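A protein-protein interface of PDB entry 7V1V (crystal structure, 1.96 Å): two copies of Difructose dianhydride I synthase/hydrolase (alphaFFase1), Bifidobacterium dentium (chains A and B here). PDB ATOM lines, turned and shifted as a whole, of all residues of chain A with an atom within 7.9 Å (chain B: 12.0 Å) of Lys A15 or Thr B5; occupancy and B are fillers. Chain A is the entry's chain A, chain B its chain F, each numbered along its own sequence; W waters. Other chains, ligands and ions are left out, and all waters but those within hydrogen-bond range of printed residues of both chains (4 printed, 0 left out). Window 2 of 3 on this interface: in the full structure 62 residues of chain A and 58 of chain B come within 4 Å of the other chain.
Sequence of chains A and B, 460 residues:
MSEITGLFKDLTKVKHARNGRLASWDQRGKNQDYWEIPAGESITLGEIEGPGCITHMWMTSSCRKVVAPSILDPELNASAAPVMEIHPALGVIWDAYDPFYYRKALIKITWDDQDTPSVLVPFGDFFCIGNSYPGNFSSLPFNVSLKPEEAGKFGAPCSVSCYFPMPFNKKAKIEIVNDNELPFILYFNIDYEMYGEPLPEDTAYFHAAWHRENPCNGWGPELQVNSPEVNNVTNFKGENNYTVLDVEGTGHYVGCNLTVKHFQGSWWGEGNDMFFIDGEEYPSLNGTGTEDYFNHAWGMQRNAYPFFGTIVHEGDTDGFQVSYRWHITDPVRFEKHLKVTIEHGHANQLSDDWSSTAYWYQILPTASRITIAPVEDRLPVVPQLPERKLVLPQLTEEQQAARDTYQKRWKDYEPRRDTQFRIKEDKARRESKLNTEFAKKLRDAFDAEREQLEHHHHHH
OG1 of Thr B5 lies within hydrogen-bond range of NZ of Lys A15 (2.9 Å). The side-chain carboxylate of Asp A10 lies within hydrogen-bond range of the backbone NH of Gly B6. NZ of Lys A9 lies close to NZ of Lys B9 (3.4 Å). NZ of Lys A15 is in hydrogen-bond range of O of Glu B3 (2.7 Å). The side-chain carboxylate (OD2) of Asp A10 is in salt-bridge range of the side-chain amino group (NZ) of Lys B9 (3.8 Å).
OG1 of Thr A12 lies within hydrogen-bond range of O of Lys A9. The side-chain amino group (NZ) of Lys A13 is in salt-bridge range of the side-chain carboxylate (OD1) of Asp A10, at 2.5 Å. OD1 of Asp A10 lies within salt-bridge range of NZ of Lys A9, at 3.8 Å. The backbone carbonyl oxygen (O) of Cys A53 is in hydrogen-bond range of the backbone NH (N) of Glu A193 (2.9 Å). NZ of Lys A15 lies within salt-bridge range of OE2 of Glu A193 (2.6 Å). The backbone carbonyl oxygen (O) of Lys B9 is in hydrogen-bond range of the side-chain hydroxyl (OG1) of Thr B12, 2.7 Å away.
Among the printed residues, pairs that only touch across the chains: Tyr A195 with Ile B4 (3.1 Å), Pro A165 with Phe B8 (3.4 Å), Asp A10 with Thr B5 (3.4 Å), Tyr A195 with Glu B3 (3.5 Å), Cys A53 with Ile B4 (3.8 Å), Leu A199 with Glu B3 (3.9 Å), Pro A165 with Thr B12 (3.9 Å) and Leu A199 with Ile B4 (3.9 Å).
Printed residues of chain B within 4 Å of Lys A15: Glu B3 (2.7 Å) and Thr B5 (2.9 Å). No residue of chain B comes within 4 Å of Lys A13. No residue of chain B comes within 4 Å of His A16. No residue of chain B comes within 4 Å of Ala A17. Glu A193 touches none of the printed residues of chain B. Of the printed residues of chain A, Gly B6 touches Asp A10. Of the printed residues of chain A, Lys B9 touches Lys A9 (3.4 Å) and Asp A10 (3.7 Å). Of the printed residues of chain A, Thr B12 touches Pro A165. Thr A55 touches none of the printed residues of chain B. The nearest printed residue of chain B that does not touch Cys A53 is Thr B12 (5.3 Å).
Of the 11 printed residues of chain B, 7 touch a printed residue of chain A. Hydrophobic or aromatic side chains of chain B that line the printed part of chain A: Ile B4 and Phe B8. Of the 20 printed residues of chain A, 7 touch a printed residue of chain B. Hydrophobic or aromatic side chains of chain A within 4 Å of the printed part of chain B: Pro A165, Tyr A195 and Leu A199. Among the printed residues, Asp or Glu carboxylates within 4 Å of a Lys or Arg side-chain nitrogen of the other chain: Asp A10 with Lys B9 (3.8 Å).
Lys A9 touches its own counterpart, Lys B9. Asp A10 touches Lys B9, but with the chains exchanged Lys A9 does not touch Asp B10 (7.1 Å). 6 positions are printed for both chains. Of the 13 pairs that touch across the chains among the printed residues, 1 has its exchanged pair printed and touching as well.
Water W2 bridges O of Leu A7 (2.6 Å) and N of Leu B7 (3.0 Å). Water W3 lies within hydrogen-bond range of OE2 of Glu A193, N of Thr B5 and NZ of Lys A15. Water W1 lies within hydrogen-bond range of the backbone carbonyl oxygen (O) of His A16 and the side-chain carboxylate (OE2) of Glu B3. Water W4 lies within hydrogen-bond range of the side-chain carboxylate of Asp A10, the backbone carbonyl oxygen of Gly B6 and the side-chain amino group of Lys A9.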
ATOM      1  N   LEU A   7       8.394  38.073  -1.983  1.00  0.00           N
ATOM      2  CA  LEU A   7       8.061  37.226  -0.815  1.00  0.00           C
ATOM      3  C   LEU A   7       6.675  37.579  -0.246  1.00  0.00           C
ATOM      4  O   LEU A   7       6.141  36.732   0.519  1.00  0.00           O
ATOM      5  CB  LEU A   7       9.169  37.360   0.238  1.00  0.00           C
ATOM      6  CG  LEU A   7       9.377  38.755   0.836  1.00  0.00           C
ATOM      7  CD1 LEU A   7       8.587  38.936   2.123  1.00  0.00           C
ATOM      8  CD2 LEU A   7      10.850  38.997   1.105  1.00  0.00           C
ATOM      9  N   LYS A   9       4.007  38.139  -2.166  1.00  0.00           N
ATOM     10  CA  LYS A   9       3.011  38.058  -3.267  1.00  0.00           C
ATOM     11  C   LYS A   9       1.782  37.252  -2.816  1.00  0.00           C
ATOM     12  O   LYS A   9       0.706  37.565  -3.275  1.00  0.00           O
ATOM     13  CB  LYS A   9       3.617  37.507  -4.556  1.00  0.00           C
ATOM     14  CG  LYS A   9       3.919  36.028  -4.578  1.00  0.00           C
ATOM     15  CD  LYS A   9       4.414  35.565  -5.941  1.00  0.00           C
ATOM     16  CE  LYS A   9       5.522  34.547  -5.822  1.00  0.00           C
ATOM     17  NZ  LYS A   9       5.191  33.474  -4.842  1.00  0.00           N
ATOM     18  N   ASP A  10       1.922  36.246  -1.961  1.00  0.00           N
ATOM     19  CA  ASP A  10       0.773  35.358  -1.640  1.00  0.00           C
ATOM     20  C   ASP A  10      -0.285  36.113  -0.825  1.00  0.00           C
ATOM     21  O   ASP A  10      -1.407  35.611  -0.761  1.00  0.00           O
ATOM     22  CB  ASP A  10       1.229  34.052  -1.013  1.00  0.00           C
ATOM     23  CG  ASP A  10       1.901  33.128  -2.011  1.00  0.00           C
ATOM     24  OD1 ASP A  10       1.721  33.346  -3.223  1.00  0.00           O
ATOM     25  OD2 ASP A  10       2.601  32.206  -1.574  1.00  0.00           O
ATOM     26  N   LEU A  11       0.015  37.302  -0.284  1.00  0.00           N
ATOM     27  CA  LEU A  11      -1.005  38.155   0.393  1.00  0.00           C
ATOM     28  C   LEU A  11      -2.014  38.711  -0.623  1.00  0.00           C
ATOM     29  O   LEU A  11      -3.082  39.167  -0.201  1.00  0.00           O
ATOM     30  CB  LEU A  11      -0.321  39.331   1.105  1.00  0.00           C
ATOM     31  CG  LEU A  11       0.657  38.986   2.222  1.00  0.00           C
ATOM     32  CD1 LEU A  11       1.138  40.274   2.880  1.00  0.00           C
ATOM     33  CD2 LEU A  11       0.052  38.036   3.245  1.00  0.00           C
ATOM     34  N   THR A  12      -1.695  38.731  -1.907  1.00  0.00           N
ATOM     35  CA  THR A  12      -2.550  39.396  -2.926  1.00  0.00           C
ATOM     36  C   THR A  12      -3.457  38.394  -3.644  1.00  0.00           C
ATOM     37  O   THR A  12      -4.046  38.785  -4.644  1.00  0.00           O
ATOM     38  CB  THR A  12      -1.705  40.155  -3.947  1.00  0.00           C
ATOM     39  OG1 THR A  12      -0.954  39.173  -4.669  1.00  0.00           O
ATOM     40  CG2 THR A  12      -0.825  41.177  -3.262  1.00  0.00           C
ATOM     41  N   LYS A  13      -3.608  37.177  -3.134  1.00  0.00           N
ATOM     42  CA  LYS A  13      -4.599  36.217  -3.682  1.00  0.00           C
ATOM     43  C   LYS A  13      -5.290  35.453  -2.544  1.00  0.00           C
ATOM     44  O   LYS A  13      -4.645  35.140  -1.537  1.00  0.00           O
ATOM     45  CB  LYS A  13      -3.923  35.263  -4.662  1.00  0.00           C
ATOM     46  CG  LYS A  13      -2.745  34.496  -4.092  1.00  0.00           C
ATOM     47  CD  LYS A  13      -2.270  33.366  -5.013  1.00  0.00           C
ATOM     48  CE  LYS A  13      -0.889  32.862  -4.653  1.00  0.00           C
ATOM     49  NZ  LYS A  13       0.149  33.851  -5.035  1.00  0.00           N
ATOM     50  N   VAL A  14      -6.584  35.203  -2.678  1.00  0.00           N
ATOM     51  CA  VAL A  14      -7.365  34.533  -1.610  1.00  0.00           C
ATOM     52  C   VAL A  14      -7.135  33.022  -1.746  1.00  0.00           C
ATOM     53  O   VAL A  14      -6.862  32.534  -2.853  1.00  0.00           O
ATOM     54  CB  VAL A  14      -8.854  34.933  -1.633  1.00  0.00           C
ATOM     55  CG1 VAL A  14      -9.011  36.443  -1.513  1.00  0.00           C
ATOM     56  CG2 VAL A  14      -9.601  34.409  -2.841  1.00  0.00           C
ATOM     57  N   LYS A  15      -7.193  32.315  -0.635  1.00  0.00           N
ATOM     58  CA  LYS A  15      -7.146  30.841  -0.603  1.00  0.00           C
ATOM     59  C   LYS A  15      -8.400  30.366   0.131  1.00  0.00           C
ATOM     60  O   LYS A  15      -8.773  30.975   1.156  1.00  0.00           O
ATOM     61  CB  LYS A  15      -5.857  30.379   0.078  1.00  0.00           C
ATOM     62  CG  LYS A  15      -5.630  28.883   0.013  1.00  0.00           C
ATOM     63  CD  LYS A  15      -4.643  28.379   1.043  1.00  0.00           C
ATOM     64  CE  LYS A  15      -3.265  28.987   0.889  1.00  0.00           C
ATOM     65  NZ  LYS A  15      -2.310  28.476   1.906  1.00  0.00           N
ATOM     66  N   HIS A  16      -9.026  29.307  -0.366  1.00  0.00           N
ATOM     67  CA  HIS A  16     -10.248  28.729   0.243  1.00  0.00           C
ATOM     68  C   HIS A  16      -9.790  27.682   1.251  1.00  0.00           C
ATOM     69  O   HIS A  16      -9.968  26.494   0.977  1.00  0.00           O
ATOM     70  CB  HIS A  16     -11.232  28.286  -0.863  1.00  0.00           C
ATOM     71  CG  HIS A  16     -11.629  29.447  -1.723  1.00  0.00           C
ATOM     72  ND1 HIS A  16     -12.585  30.383  -1.332  1.00  0.00           N
ATOM     73  CD2 HIS A  16     -11.133  29.902  -2.899  1.00  0.00           C
ATOM     74  CE1 HIS A  16     -12.697  31.322  -2.267  1.00  0.00           C
ATOM     75  NE2 HIS A  16     -11.809  31.051  -3.232  1.00  0.00           N
ATOM     76  N   ALA A  17      -9.159  28.149   2.337  1.00  0.00           N
ATOM     77  CA  ALA A  17      -8.637  27.334   3.462  1.00  0.00           C
ATOM     78  C   ALA A  17      -9.139  27.918   4.780  1.00  0.00           C
ATOM     79  O   ALA A  17      -9.250  29.152   4.877  1.00  0.00           O
ATOM     80  CB  ALA A  17      -7.134  27.292   3.450  1.00  0.00           C
ATOM     81  N   ARG A  18      -9.405  27.046   5.756  1.00  0.00           N
ATOM     82  CA  ARG A  18     -10.121  27.386   7.005  1.00  0.00           C
ATOM     83  C   ARG A  18      -9.112  27.349   8.151  1.00  0.00           C
ATOM     84  O   ARG A  18      -8.475  26.310   8.368  1.00  0.00           O
ATOM     85  CB  ARG A  18     -11.292  26.436   7.252  1.00  0.00           C
ATOM     86  CG  ARG A  18     -12.018  26.641   8.576  1.00  0.00           C
ATOM     87  CD  ARG A  18     -12.602  28.016   8.740  1.00  0.00           C
ATOM     88  NE  ARG A  18     -13.740  28.125   9.644  1.00  0.00           N
ATOM     89  CZ  ARG A  18     -13.698  28.403  10.943  1.00  0.00           C
ATOM     90  NH1 ARG A  18     -12.552  28.573  11.577  1.00  0.00           N
ATOM     91  NH2 ARG A  18     -14.826  28.557  11.615  1.00  0.00           N
ATOM     92  N   ASN A  19      -8.975  28.468   8.848  1.00  0.00           N
ATOM     93  CA  ASN A  19      -8.096  28.553  10.037  1.00  0.00           C
ATOM     94  C   ASN A  19      -8.647  27.663  11.145  1.00  0.00           C
ATOM     95  O   ASN A  19      -9.907  27.586  11.328  1.00  0.00           O
ATOM     96  CB  ASN A  19      -7.962  29.970  10.596  1.00  0.00           C
ATOM     97  CG  ASN A  19      -6.995  30.790   9.785  1.00  0.00           C
ATOM     98  OD1 ASN A  19      -5.912  31.166  10.262  1.00  0.00           O
ATOM     99  ND2 ASN A  19      -7.414  31.128   8.591  1.00  0.00           N
ATOM    100  N   CYS A  53      -1.990  22.340   7.307  1.00  0.00           N
ATOM    101  CA  CYS A  53      -0.608  22.809   7.494  1.00  0.00           C
ATOM    102  C   CYS A  53      -0.531  23.630   8.781  1.00  0.00           C
ATOM    103  O   CYS A  53      -1.358  24.553   8.933  1.00  0.00           O
ATOM    104  CB  CYS A  53      -0.174  23.629   6.290  1.00  0.00           C
ATOM    105  SG  CYS A  53       1.590  24.020   6.284  1.00  0.00           S
ATOM    106  N   THR A  55       0.990  26.599  10.718  1.00  0.00           N
ATOM    107  CA  THR A  55       1.584  27.844  10.170  1.00  0.00           C
ATOM    108  C   THR A  55       2.350  28.620  11.233  1.00  0.00           C
ATOM    109  O   THR A  55       3.135  29.511  10.872  1.00  0.00           O
ATOM    110  CB  THR A  55       0.492  28.743   9.597  1.00  0.00           C
ATOM    111  OG1 THR A  55      -0.411  29.008  10.672  1.00  0.00           O
ATOM    112  CG2 THR A  55      -0.201  28.094   8.420  1.00  0.00           C
ATOM    113  N   PRO A 165       6.581  25.950   8.327  1.00  0.00           N
ATOM    114  CA  PRO A 165       5.312  25.291   8.004  1.00  0.00           C
ATOM    115  C   PRO A 165       5.396  23.767   8.139  1.00  0.00           C
ATOM    116  O   PRO A 165       6.434  23.173   7.839  1.00  0.00           O
ATOM    117  CB  PRO A 165       5.070  25.710   6.549  1.00  0.00           C
ATOM    118  CG  PRO A 165       6.466  25.821   6.005  1.00  0.00           C
ATOM    119  CD  PRO A 165       7.246  26.475   7.131  1.00  0.00           C
ATOM    120  N   GLU A 193      -3.999  25.767   8.999  1.00  0.00           N
ATOM    121  CA  GLU A 193      -5.114  25.907   8.052  1.00  0.00           C
ATOM    122  C   GLU A 193      -5.463  24.510   7.551  1.00  0.00           C
ATOM    123  O   GLU A 193      -4.589  23.634   7.533  1.00  0.00           O
ATOM    124  CB  GLU A 193      -4.830  26.986   7.010  1.00  0.00           C
ATOM    125  CG  GLU A 193      -3.520  26.848   6.303  1.00  0.00           C
ATOM    126  CD  GLU A 193      -3.220  27.961   5.310  1.00  0.00           C
ATOM    127  OE1 GLU A 193      -3.639  29.118   5.520  1.00  0.00           O
ATOM    128  OE2 GLU A 193      -2.542  27.654   4.345  1.00  0.00           O
ATOM    129  N   MET A 194      -6.736  24.330   7.232  1.00  0.00           N
ATOM    130  CA  MET A 194      -7.284  23.096   6.632  1.00  0.00           C
ATOM    131  C   MET A 194      -7.616  23.386   5.171  1.00  0.00           C
ATOM    132  O   MET A 194      -8.132  24.483   4.870  1.00  0.00           O
ATOM    133  CB  MET A 194      -8.540  22.661   7.386  1.00  0.00           C
ATOM    134  CG  MET A 194      -8.298  22.408   8.860  1.00  0.00           C
ATOM    135  SD  MET A 194      -9.806  21.825   9.637  1.00  0.00           S
ATOM    136  CE  MET A 194     -10.826  23.288   9.614  1.00  0.00           C
ATOM    137  N   TYR A 195      -7.379  22.405   4.321  1.00  0.00           N
ATOM    138  CA  TYR A 195      -7.582  22.476   2.852  1.00  0.00           C
ATOM    139  C   TYR A 195      -8.735  21.574   2.429  1.00  0.00           C
ATOM    140  O   TYR A 195      -9.010  20.601   3.132  1.00  0.00           O
ATOM    141  CB  TYR A 195      -6.283  22.067   2.174  1.00  0.00           C
ATOM    142  CG  TYR A 195      -5.096  22.877   2.631  1.00  0.00           C
ATOM    143  CD1 TYR A 195      -5.133  24.264   2.604  1.00  0.00           C
ATOM    144  CD2 TYR A 195      -3.937  22.262   3.068  1.00  0.00           C
ATOM    145  CE1 TYR A 195      -4.057  25.022   3.043  1.00  0.00           C
ATOM    146  CE2 TYR A 195      -2.853  23.004   3.504  1.00  0.00           C
ATOM    147  CZ  TYR A 195      -2.909  24.389   3.488  1.00  0.00           C
ATOM    148  OH  TYR A 195      -1.819  25.109   3.883  1.00  0.00           O
ATOM    149  N   LEU A 199      -3.067  17.652  -0.374  1.00  0.00           N
ATOM    150  CA  LEU A 199      -1.774  18.234  -0.797  1.00  0.00           C
ATOM    151  C   LEU A 199      -1.147  17.272  -1.794  1.00  0.00           C
ATOM    152  O   LEU A 199      -1.419  16.086  -1.708  1.00  0.00           O
ATOM    153  CB  LEU A 199      -0.888  18.382   0.439  1.00  0.00           C
ATOM    154  CG  LEU A 199      -1.447  19.346   1.483  1.00  0.00           C
ATOM    155  CD1 LEU A 199      -0.617  19.342   2.740  1.00  0.00           C
ATOM    156  CD2 LEU A 199      -1.523  20.736   0.900  1.00  0.00           C
ATOM    157  N   PHE A 446     -16.199  22.508   8.092  1.00  0.00           N
ATOM    158  CA  PHE A 446     -15.464  22.986   6.892  1.00  0.00           C
ATOM    159  C   PHE A 446     -15.775  22.077   5.692  1.00  0.00           C
ATOM    160  O   PHE A 446     -16.161  22.583   4.614  1.00  0.00           O
ATOM    161  CB  PHE A 446     -13.954  23.045   7.132  1.00  0.00           C
ATOM    162  CG  PHE A 446     -13.167  23.521   5.935  1.00  0.00           C
ATOM    163  CD1 PHE A 446     -13.553  24.654   5.223  1.00  0.00           C
ATOM    164  CD2 PHE A 446     -12.022  22.851   5.533  1.00  0.00           C
ATOM    165  CE1 PHE A 446     -12.833  25.082   4.116  1.00  0.00           C
ATOM    166  CE2 PHE A 446     -11.308  23.282   4.424  1.00  0.00           C
ATOM    167  CZ  PHE A 446     -11.714  24.390   3.722  1.00  0.00           C
ATOM    168  N   GLU B   3      -0.810  24.903  -2.905  1.00  0.00           N
ATOM    169  CA  GLU B   3      -1.774  25.064  -1.759  1.00  0.00           C
ATOM    170  C   GLU B   3      -1.098  25.660  -0.512  1.00  0.00           C
ATOM    171  O   GLU B   3      -1.773  26.439   0.180  1.00  0.00           O
ATOM    172  CB  GLU B   3      -2.417  23.744  -1.351  1.00  0.00           C
ATOM    173  CG  GLU B   3      -3.701  23.973  -0.567  1.00  0.00           C
ATOM    174  CD  GLU B   3      -4.905  24.286  -1.439  1.00  0.00           C
ATOM    175  OE1 GLU B   3      -5.265  23.399  -2.224  1.00  0.00           O
ATOM    176  OE2 GLU B   3      -5.470  25.415  -1.344  1.00  0.00           O
ATOM    177  N   ILE B   4       0.135  25.265  -0.178  1.00  0.00           N
ATOM    178  CA  ILE B   4       0.926  25.968   0.881  1.00  0.00           C
ATOM    179  C   ILE B   4       1.324  27.326   0.297  1.00  0.00           C
ATOM    180  O   ILE B   4       1.721  27.367  -0.883  1.00  0.00           O
ATOM    181  CB  ILE B   4       2.151  25.158   1.345  1.00  0.00           C
ATOM    182  CG1 ILE B   4       1.787  23.721   1.742  1.00  0.00           C
ATOM    183  CG2 ILE B   4       2.896  25.884   2.458  1.00  0.00           C
ATOM    184  CD1 ILE B   4       0.513  23.587   2.537  1.00  0.00           C
ATOM    185  N   THR B   5       1.177  28.407   1.054  1.00  0.00           N
ATOM    186  CA  THR B   5       1.522  29.764   0.563  1.00  0.00           C
ATOM    187  C   THR B   5       2.523  30.413   1.527  1.00  0.00           C
ATOM    188  O   THR B   5       2.774  29.838   2.618  1.00  0.00           O
ATOM    189  CB  THR B   5       0.262  30.600   0.318  1.00  0.00           C
ATOM    190  OG1 THR B   5      -0.456  30.687   1.545  1.00  0.00           O
ATOM    191  CG2 THR B   5      -0.596  30.007  -0.773  1.00  0.00           C
ATOM    192  N   GLY B   6       3.122  31.529   1.093  1.00  0.00           N
ATOM    193  CA  GLY B   6       4.041  32.356   1.898  1.00  0.00           C
ATOM    194  C   GLY B   6       5.502  32.030   1.655  1.00  0.00           C
ATOM    195  O   GLY B   6       5.819  31.058   0.931  1.00  0.00           O
ATOM    196  N   LEU B   7       6.383  32.786   2.302  1.00  0.00           N
ATOM    197  CA  LEU B   7       7.816  32.818   1.949  1.00  0.00           C
ATOM    198  C   LEU B   7       8.512  31.513   2.358  1.00  0.00           C
ATOM    199  O   LEU B   7       9.596  31.283   1.835  1.00  0.00           O
ATOM    200  CB  LEU B   7       8.458  34.073   2.547  1.00  0.00           C
ATOM    201  CG  LEU B   7       8.529  34.143   4.069  1.00  0.00           C
ATOM    202  CD1 LEU B   7       9.840  33.542   4.556  1.00  0.00           C
ATOM    203  CD2 LEU B   7       8.371  35.585   4.528  1.00  0.00           C
ATOM    204  N   PHE B   8       7.922  30.669   3.214  1.00  0.00           N
ATOM    205  CA  PHE B   8       8.537  29.356   3.565  1.00  0.00           C
ATOM    206  C   PHE B   8       8.014  28.232   2.658  1.00  0.00           C
ATOM    207  O   PHE B   8       8.421  27.070   2.870  1.00  0.00           O
ATOM    208  CB  PHE B   8       8.246  28.953   5.013  1.00  0.00           C
ATOM    209  CG  PHE B   8       8.741  29.926   6.054  1.00  0.00           C
ATOM    210  CD1 PHE B   8      10.070  29.923   6.445  1.00  0.00           C
ATOM    211  CD2 PHE B   8       7.868  30.827   6.668  1.00  0.00           C
ATOM    212  CE1 PHE B   8      10.530  30.800   7.421  1.00  0.00           C
ATOM    213  CE2 PHE B   8       8.338  31.733   7.613  1.00  0.00           C
ATOM    214  CZ  PHE B   8       9.670  31.717   7.985  1.00  0.00           C
ATOM    215  N   LYS B   9       7.136  28.526   1.706  1.00  0.00           N
ATOM    216  CA  LYS B   9       6.331  27.470   1.029  1.00  0.00           C
ATOM    217  C   LYS B   9       7.219  26.479   0.271  1.00  0.00           C
ATOM    218  O   LYS B   9       6.859  25.319   0.247  1.00  0.00           O
ATOM    219  CB  LYS B   9       5.281  28.074   0.096  1.00  0.00           C
ATOM    220  CG  LYS B   9       5.798  28.576  -1.246  1.00  0.00           C
ATOM    221  CD  LYS B   9       4.733  29.215  -2.111  1.00  0.00           C
ATOM    222  CE  LYS B   9       5.137  29.273  -3.574  1.00  0.00           C
ATOM    223  NZ  LYS B   9       4.317  30.250  -4.330  1.00  0.00           N
ATOM    224  N   ASP B  10       8.328  26.893  -0.346  1.00  0.00           N
ATOM    225  CA  ASP B  10       9.158  25.938  -1.142  1.00  0.00           C
ATOM    226  C   ASP B  10       9.863  24.930  -0.231  1.00  0.00           C
ATOM    227  O   ASP B  10      10.348  23.916  -0.778  1.00  0.00           O
ATOM    228  CB  ASP B  10      10.168  26.638  -2.041  1.00  0.00           C
ATOM    229  CG  ASP B  10       9.525  27.452  -3.157  1.00  0.00           C
ATOM    230  OD1 ASP B  10       8.337  27.222  -3.462  1.00  0.00           O
ATOM    231  OD2 ASP B  10      10.200  28.331  -3.677  1.00  0.00           O
ATOM    232  N   LEU B  11       9.879  25.132   1.099  1.00  0.00           N
ATOM    233  CA  LEU B  11      10.398  24.088   2.015  1.00  0.00           C
ATOM    234  C   LEU B  11       9.514  22.830   1.990  1.00  0.00           C
ATOM    235  O   LEU B  11       9.991  21.791   2.504  1.00  0.00           O
ATOM    236  CB  LEU B  11      10.508  24.634   3.432  1.00  0.00           C
ATOM    237  CG  LEU B  11      11.524  25.763   3.620  1.00  0.00           C
ATOM    238  CD1 LEU B  11      11.674  26.034   5.093  1.00  0.00           C
ATOM    239  CD2 LEU B  11      12.867  25.427   3.016  1.00  0.00           C
ATOM    240  N   THR B  12       8.265  22.928   1.513  1.00  0.00           N
ATOM    241  CA  THR B  12       7.257  21.836   1.607  1.00  0.00           C
ATOM    242  C   THR B  12       7.212  21.024   0.297  1.00  0.00           C
ATOM    243  O   THR B  12       6.329  20.170   0.185  1.00  0.00           O
ATOM    244  CB  THR B  12       5.868  22.362   1.965  1.00  0.00           C
ATOM    245  OG1 THR B  12       5.353  23.140   0.879  1.00  0.00           O
ATOM    246  CG2 THR B  12       5.885  23.179   3.242  1.00  0.00           C
ATOM    247  N   LYS B  13       8.147  21.235  -0.623  1.00  0.00           N
ATOM    248  CA  LYS B  13       8.223  20.454  -1.888  1.00  0.00           C
ATOM    249  C   LYS B  13       9.675  20.109  -2.203  1.00  0.00           C
ATOM    250  O   LYS B  13      10.574  20.924  -1.956  1.00  0.00           O
ATOM    251  CB  LYS B  13       7.507  21.152  -3.046  1.00  0.00           C
ATOM    252  CG  LYS B  13       7.651  22.661  -3.127  1.00  0.00           C
ATOM    253  CD  LYS B  13       6.408  23.326  -3.703  1.00  0.00           C
ATOM    254  CE  LYS B  13       6.559  24.818  -3.928  1.00  0.00           C
ATOM    255  NZ  LYS B  13       7.744  25.121  -4.771  1.00  0.00           N
HETATM  256  O   HOH W   1      -8.079  24.554   0.488  1.00  0.00           O
HETATM  257  O   HOH W   2       5.382  35.573   2.717  1.00  0.00           O
HETATM  258  O   HOH W   3       0.049  28.125   3.796  1.00  0.00           O
HETATM  259  O   HOH W   4       5.613  32.705  -1.654  1.00  0.00           O
